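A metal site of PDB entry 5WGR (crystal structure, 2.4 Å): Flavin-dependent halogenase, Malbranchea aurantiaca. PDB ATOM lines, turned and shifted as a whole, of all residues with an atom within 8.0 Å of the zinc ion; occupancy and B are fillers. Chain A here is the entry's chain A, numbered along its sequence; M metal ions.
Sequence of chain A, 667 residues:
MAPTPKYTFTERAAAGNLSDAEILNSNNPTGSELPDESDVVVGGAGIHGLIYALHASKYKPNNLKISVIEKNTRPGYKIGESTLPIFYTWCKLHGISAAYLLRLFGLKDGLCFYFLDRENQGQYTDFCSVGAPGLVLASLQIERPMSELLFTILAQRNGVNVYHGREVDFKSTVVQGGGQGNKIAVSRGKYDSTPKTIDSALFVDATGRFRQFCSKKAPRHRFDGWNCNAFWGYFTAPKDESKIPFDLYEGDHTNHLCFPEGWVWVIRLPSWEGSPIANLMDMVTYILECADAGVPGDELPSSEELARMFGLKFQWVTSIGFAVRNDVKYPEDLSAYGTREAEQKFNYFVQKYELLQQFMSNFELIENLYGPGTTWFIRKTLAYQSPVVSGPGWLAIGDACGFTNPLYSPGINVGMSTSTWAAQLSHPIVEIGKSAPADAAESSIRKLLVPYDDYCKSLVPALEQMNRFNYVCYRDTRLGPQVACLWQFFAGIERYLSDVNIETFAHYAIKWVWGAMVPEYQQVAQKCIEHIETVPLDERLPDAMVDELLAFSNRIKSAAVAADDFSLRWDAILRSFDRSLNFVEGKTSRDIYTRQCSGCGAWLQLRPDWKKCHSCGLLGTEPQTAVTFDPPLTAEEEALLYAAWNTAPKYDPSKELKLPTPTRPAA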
ATOM      1  N   ARG A 268      21.941  -0.345 -11.529  1.00  0.00           N
ATOM      2  CA  ARG A 268      20.551  -0.003 -11.212  1.00  0.00           C
ATOM      3  C   ARG A 268      19.796  -1.286 -10.856  1.00  0.00           C
ATOM      4  O   ARG A 268      19.771  -2.230 -11.649  1.00  0.00           O
ATOM      5  CB  ARG A 268      19.906   0.710 -12.400  1.00  0.00           C
ATOM      6  CG  ARG A 268      18.493   1.213 -12.151  1.00  0.00           C
ATOM      7  CD  ARG A 268      17.763   1.540 -13.432  1.00  0.00           C
ATOM      8  NE  ARG A 268      16.310   1.505 -13.224  1.00  0.00           N
ATOM      9  CZ  ARG A 268      15.552   2.587 -13.079  1.00  0.00           C
ATOM     10  NH1 ARG A 268      16.092   3.800 -13.136  1.00  0.00           N
ATOM     11  NH2 ARG A 268      14.244   2.462 -12.886  1.00  0.00           N
ATOM     12  N   SER A 302       2.818  -7.059 -11.747  1.00  0.00           N
ATOM     13  CA  SER A 302       4.056  -6.291 -11.777  1.00  0.00           C
ATOM     14  C   SER A 302       4.679  -6.233 -10.389  1.00  0.00           C
ATOM     15  O   SER A 302       4.034  -6.494  -9.371  1.00  0.00           O
ATOM     16  CB  SER A 302       3.797  -4.874 -12.303  1.00  0.00           C
ATOM     17  OG  SER A 302       3.097  -4.090 -11.356  1.00  0.00           O
ATOM     18  N   GLU A 304       5.443  -3.767  -8.547  1.00  0.00           N
ATOM     19  CA  GLU A 304       4.741  -2.891  -7.615  1.00  0.00           C
ATOM     20  C   GLU A 304       3.419  -3.502  -7.167  1.00  0.00           C
ATOM     21  O   GLU A 304       3.022  -3.317  -6.013  1.00  0.00           O
ATOM     22  CB  GLU A 304       4.525  -1.517  -8.245  1.00  0.00           C
ATOM     23  CG  GLU A 304       5.834  -0.759  -8.473  1.00  0.00           C
ATOM     24  CD  GLU A 304       5.630   0.552  -9.212  1.00  0.00           C
ATOM     25  OE1 GLU A 304       4.476   1.014  -9.313  1.00  0.00           O
ATOM     26  OE2 GLU A 304       6.639   1.122  -9.706  1.00  0.00           O
ATOM     27  N   TRP A 316      13.544   1.838  -6.346  1.00  0.00           N
ATOM     28  CA  TRP A 316      14.668   1.745  -7.259  1.00  0.00           C
ATOM     29  C   TRP A 316      15.873   2.462  -6.652  1.00  0.00           C
ATOM     30  O   TRP A 316      15.765   3.610  -6.219  1.00  0.00           O
ATOM     31  CB  TRP A 316      14.315   2.348  -8.612  1.00  0.00           C
ATOM     32  CG  TRP A 316      13.459   1.434  -9.419  1.00  0.00           C
ATOM     33  CD1 TRP A 316      12.107   1.493  -9.578  1.00  0.00           C
ATOM     34  CD2 TRP A 316      13.896   0.280 -10.150  1.00  0.00           C
ATOM     35  NE1 TRP A 316      11.683   0.453 -10.380  1.00  0.00           N
ATOM     36  CE2 TRP A 316      12.761  -0.300 -10.735  1.00  0.00           C
ATOM     37  CE3 TRP A 316      15.150  -0.304 -10.371  1.00  0.00           C
ATOM     38  CZ2 TRP A 316      12.841  -1.445 -11.534  1.00  0.00           C
ATOM     39  CZ3 TRP A 316      15.231  -1.440 -11.165  1.00  0.00           C
ATOM     40  CH2 TRP A 316      14.077  -1.993 -11.736  1.00  0.00           C
ATOM     41  N   ARG A 595      14.182  -1.055 -23.602  1.00  0.00           N
ATOM     42  CA  ARG A 595      13.531   0.258 -23.610  1.00  0.00           C
ATOM     43  C   ARG A 595      13.230   0.621 -22.160  1.00  0.00           C
ATOM     44  O   ARG A 595      13.078  -0.265 -21.306  1.00  0.00           O
ATOM     45  CB  ARG A 595      12.249   0.296 -24.445  1.00  0.00           C
ATOM     46  CG  ARG A 595      10.999  -0.199 -23.695  1.00  0.00           C
ATOM     47  CD  ARG A 595       9.711   0.073 -24.470  1.00  0.00           C
ATOM     48  NE  ARG A 595       8.566  -0.565 -23.819  1.00  0.00           N
ATOM     49  CZ  ARG A 595       7.693   0.058 -23.038  1.00  0.00           C
ATOM     50  NH1 ARG A 595       7.810   1.357 -22.806  1.00  0.00           N
ATOM     51  NH2 ARG A 595       6.682  -0.619 -22.503  1.00  0.00           N
ATOM     52  N   GLN A 596      13.124   1.911 -21.899  1.00  0.00           N
ATOM     53  CA  GLN A 596      12.861   2.425 -20.563  1.00  0.00           C
ATOM     54  C   GLN A 596      11.393   2.785 -20.420  1.00  0.00           C
ATOM     55  O   GLN A 596      10.826   3.463 -21.291  1.00  0.00           O
ATOM     56  CB  GLN A 596      13.733   3.654 -20.268  1.00  0.00           C
ATOM     57  CG  GLN A 596      14.072   3.849 -18.816  1.00  0.00           C
ATOM     58  CD  GLN A 596      14.877   5.108 -18.545  1.00  0.00           C
ATOM     59  OE1 GLN A 596      15.222   5.842 -19.471  1.00  0.00           O
ATOM     60  NE2 GLN A 596      15.162   5.373 -17.280  1.00  0.00           N
ATOM     61  N   CYS A 597      10.759   2.315 -19.352  1.00  0.00           N
ATOM     62  CA  CYS A 597       9.350   2.591 -19.136  1.00  0.00           C
ATOM     63  C   CYS A 597       9.139   4.078 -18.883  1.00  0.00           C
ATOM     64  O   CYS A 597       9.775   4.664 -18.007  1.00  0.00           O
ATOM     65  CB  CYS A 597       8.803   1.782 -17.960  1.00  0.00           C
ATOM     66  SG  CYS A 597       7.047   2.076 -17.618  1.00  0.00           S
ATOM     67  N   SER A 598       8.272   4.700 -19.681  1.00  0.00           N
ATOM     68  CA  SER A 598       8.011   6.122 -19.509  1.00  0.00           C
ATOM     69  C   SER A 598       7.389   6.426 -18.153  1.00  0.00           C
ATOM     70  O   SER A 598       7.536   7.545 -17.651  1.00  0.00           O
ATOM     71  CB  SER A 598       7.115   6.631 -20.637  1.00  0.00           C
ATOM     72  OG  SER A 598       6.055   5.719 -20.900  1.00  0.00           O
ATOM     73  N   GLY A 599       6.712   5.443 -17.545  1.00  0.00           N
ATOM     74  CA  GLY A 599       6.028   5.644 -16.283  1.00  0.00           C
ATOM     75  C   GLY A 599       6.904   5.608 -15.044  1.00  0.00           C
ATOM     76  O   GLY A 599       6.921   6.563 -14.268  1.00  0.00           O
ATOM     77  N   CYS A 600       7.640   4.506 -14.850  1.00  0.00           N
ATOM     78  CA  CYS A 600       8.404   4.299 -13.633  1.00  0.00           C
ATOM     79  C   CYS A 600       9.918   4.369 -13.825  1.00  0.00           C
ATOM     80  O   CYS A 600      10.651   4.378 -12.821  1.00  0.00           O
ATOM     81  CB  CYS A 600       8.038   2.933 -13.014  1.00  0.00           C
ATOM     82  SG  CYS A 600       8.537   1.490 -13.986  1.00  0.00           S
ATOM     83  N   GLY A 601      10.411   4.432 -15.064  1.00  0.00           N
ATOM     84  CA  GLY A 601      11.826   4.454 -15.344  1.00  0.00           C
ATOM     85  C   GLY A 601      12.491   3.097 -15.456  1.00  0.00           C
ATOM     86  O   GLY A 601      13.692   3.042 -15.771  1.00  0.00           O
ATOM     87  N   ALA A 602      11.769   2.007 -15.225  1.00  0.00           N
ATOM     88  CA  ALA A 602      12.391   0.690 -15.246  1.00  0.00           C
ATOM     89  C   ALA A 602      12.706   0.257 -16.679  1.00  0.00           C
ATOM     90  O   ALA A 602      11.963   0.554 -17.626  1.00  0.00           O
ATOM     91  CB  ALA A 602      11.485  -0.345 -14.578  1.00  0.00           C
ATOM     92  N   TRP A 603      13.815  -0.450 -16.827  1.00  0.00           N
ATOM     93  CA  TRP A 603      14.248  -0.935 -18.126  1.00  0.00           C
ATOM     94  C   TRP A 603      13.611  -2.273 -18.450  1.00  0.00           C
ATOM     95  O   TRP A 603      13.529  -3.173 -17.597  1.00  0.00           O
ATOM     96  CB  TRP A 603      15.771  -1.028 -18.170  1.00  0.00           C
ATOM     97  CG  TRP A 603      16.414   0.323 -18.249  1.00  0.00           C
ATOM     98  CD1 TRP A 603      16.796   1.129 -17.218  1.00  0.00           C
ATOM     99  CD2 TRP A 603      16.735   1.039 -19.448  1.00  0.00           C
ATOM    100  NE1 TRP A 603      17.348   2.294 -17.692  1.00  0.00           N
ATOM    101  CE2 TRP A 603      17.319   2.267 -19.055  1.00  0.00           C
ATOM    102  CE3 TRP A 603      16.585   0.760 -20.813  1.00  0.00           C
ATOM    103  CZ2 TRP A 603      17.751   3.211 -19.984  1.00  0.00           C
ATOM    104  CZ3 TRP A 603      17.028   1.712 -21.736  1.00  0.00           C
ATOM    105  CH2 TRP A 603      17.598   2.919 -21.311  1.00  0.00           C
ATOM    106  N   LEU A 604      13.144  -2.406 -19.690  1.00  0.00           N
ATOM    107  CA  LEU A 604      12.300  -3.517 -20.121  1.00  0.00           C
ATOM    108  C   LEU A 604      12.939  -4.226 -21.299  1.00  0.00           C
ATOM    109  O   LEU A 604      13.630  -3.613 -22.109  1.00  0.00           O
ATOM    110  CB  LEU A 604      10.906  -3.023 -20.524  1.00  0.00           C
ATOM    111  CG  LEU A 604      10.179  -2.140 -19.508  1.00  0.00           C
ATOM    112  CD1 LEU A 604       8.871  -1.587 -20.089  1.00  0.00           C
ATOM    113  CD2 LEU A 604       9.908  -2.938 -18.236  1.00  0.00           C
ATOM    114  N   LYS A 612       3.151  -4.956 -21.401  1.00  0.00           N
ATOM    115  CA  LYS A 612       3.146  -4.095 -20.225  1.00  0.00           C
ATOM    116  C   LYS A 612       4.510  -4.108 -19.531  1.00  0.00           C
ATOM    117  O   LYS A 612       5.299  -5.053 -19.671  1.00  0.00           O
ATOM    118  CB  LYS A 612       2.058  -4.519 -19.237  1.00  0.00           C
ATOM    119  CG  LYS A 612       2.404  -5.761 -18.430  1.00  0.00           C
ATOM    120  CD  LYS A 612       1.401  -6.027 -17.324  1.00  0.00           C
ATOM    121  CE  LYS A 612       1.902  -7.113 -16.380  1.00  0.00           C
ATOM    122  NZ  LYS A 612       0.906  -7.439 -15.310  1.00  0.00           N
ATOM    123  N   CYS A 613       4.781  -3.028 -18.803  1.00  0.00           N
ATOM    124  CA  CYS A 613       5.959  -2.970 -17.945  1.00  0.00           C
ATOM    125  C   CYS A 613       5.841  -3.995 -16.830  1.00  0.00           C
ATOM    126  O   CYS A 613       4.818  -4.073 -16.142  1.00  0.00           O
ATOM    127  CB  CYS A 613       6.104  -1.556 -17.368  1.00  0.00           C
ATOM    128  SG  CYS A 613       7.445  -1.339 -16.170  1.00  0.00           S
ATOM    129  N   HIS A 614       6.892  -4.808 -16.649  1.00  0.00           N
ATOM    130  CA  HIS A 614       6.869  -5.828 -15.604  1.00  0.00           C
ATOM    131  C   HIS A 614       7.079  -5.263 -14.210  1.00  0.00           C
ATOM    132  O   HIS A 614       6.882  -5.982 -13.223  1.00  0.00           O
ATOM    133  CB  HIS A 614       7.937  -6.903 -15.876  1.00  0.00           C
ATOM    134  CG  HIS A 614       9.342  -6.383 -15.839  1.00  0.00           C
ATOM    135  ND1 HIS A 614      10.005  -6.109 -14.669  1.00  0.00           N
ATOM    136  CD2 HIS A 614      10.192  -6.056 -16.842  1.00  0.00           C
ATOM    137  CE1 HIS A 614      11.214  -5.654 -14.953  1.00  0.00           C
ATOM    138  NE2 HIS A 614      11.348  -5.603 -16.262  1.00  0.00           N
ATOM    139  N   SER A 615       7.474  -3.983 -14.100  1.00  0.00           N
ATOM    140  CA  SER A 615       7.784  -3.379 -12.813  1.00  0.00           C
ATOM    141  C   SER A 615       6.628  -2.554 -12.245  1.00  0.00           C
ATOM    142  O   SER A 615       6.345  -2.661 -11.045  1.00  0.00           O
ATOM    143  CB  SER A 615       9.026  -2.495 -12.936  1.00  0.00           C
ATOM    144  OG  SER A 615       9.518  -2.142 -11.653  1.00  0.00           O
ATOM    145  N   CYS A 616       5.958  -1.738 -13.066  1.00  0.00           N
ATOM    146  CA  CYS A 616       4.813  -0.976 -12.606  1.00  0.00           C
ATOM    147  C   CYS A 616       3.500  -1.342 -13.280  1.00  0.00           C
ATOM    148  O   CYS A 616       2.449  -0.835 -12.871  1.00  0.00           O
ATOM    149  CB  CYS A 616       5.063   0.526 -12.788  1.00  0.00           C
ATOM    150  SG  CYS A 616       4.779   1.101 -14.481  1.00  0.00           S
ATOM    151  N   GLY A 617       3.516  -2.200 -14.310  1.00  0.00           N
ATOM    152  CA  GLY A 617       2.296  -2.625 -14.951  1.00  0.00           C
ATOM    153  C   GLY A 617       1.760  -1.705 -16.024  1.00  0.00           C
ATOM    154  O   GLY A 617       0.736  -2.039 -16.635  1.00  0.00           O
ATOM    155  N   LEU A 618       2.396  -0.564 -16.257  1.00  0.00           N
ATOM    156  CA  LEU A 618       1.927   0.351 -17.290  1.00  0.00           C
ATOM    157  C   LEU A 618       2.031  -0.297 -18.666  1.00  0.00           C
ATOM    158  O   LEU A 618       3.038  -0.924 -19.011  1.00  0.00           O
ATOM    159  CB  LEU A 618       2.741   1.646 -17.268  1.00  0.00           C
ATOM    160  CG  LEU A 618       2.466   2.645 -18.393  1.00  0.00           C
ATOM    161  CD1 LEU A 618       1.015   3.115 -18.392  1.00  0.00           C
ATOM    162  CD2 LEU A 618       3.415   3.823 -18.286  1.00  0.00           C
ATOM    163  N   LEU A 619       0.977  -0.131 -19.456  1.00  0.00           N
ATOM    164  CA  LEU A 619       0.944  -0.708 -20.804  1.00  0.00           C
ATOM    165  C   LEU A 619       1.677   0.208 -21.764  1.00  0.00           C
ATOM    166  O   LEU A 619       1.317   1.375 -21.936  1.00  0.00           O
ATOM    167  CB  LEU A 619      -0.511  -0.905 -21.247  1.00  0.00           C
ATOM    168  CG  LEU A 619      -0.696  -1.870 -22.414  1.00  0.00           C
ATOM    169  CD1 LEU A 619      -0.341  -3.299 -21.990  1.00  0.00           C
ATOM    170  CD2 LEU A 619      -2.104  -1.799 -22.971  1.00  0.00           C
HETATM  171 ZN    ZN M   1       6.887   0.902 -15.516  1.00  0.00          ZN
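Within 4 Å of the zinc ion: Cys 597, Cys 600, Cys 613 and Cys 616.
The zinc ion is bound by SG of Cys 600, SG of Cys 616, SG of Cys 613 and SG of Cys 597.
The zinc ion has four donor atoms within binding distance.
The backbone NH (N) of Leu 618 lies close to the side-chain sulfur (SG) of Cys 616 (3.4 Å).
SG of Cys 613 lies close to N of Ser 615 (3.4 Å).
N of Cys 613 lies within hydrogen-bond range of O of Leu 618.
The backbone NH (N) of Cys 597 is in hydrogen-bond range of the backbone carbonyl oxygen (O) of Ala 602, at 2.7 Å.
The side-chain sulfur (SG) of Cys 600 lies close to the backbone NH (N) of Ala 602 (3.5 Å).
The side-chain sulfur (SG) of Cys 597 sits close to the backbone NH (N) of Gly 599 (3.4 Å).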
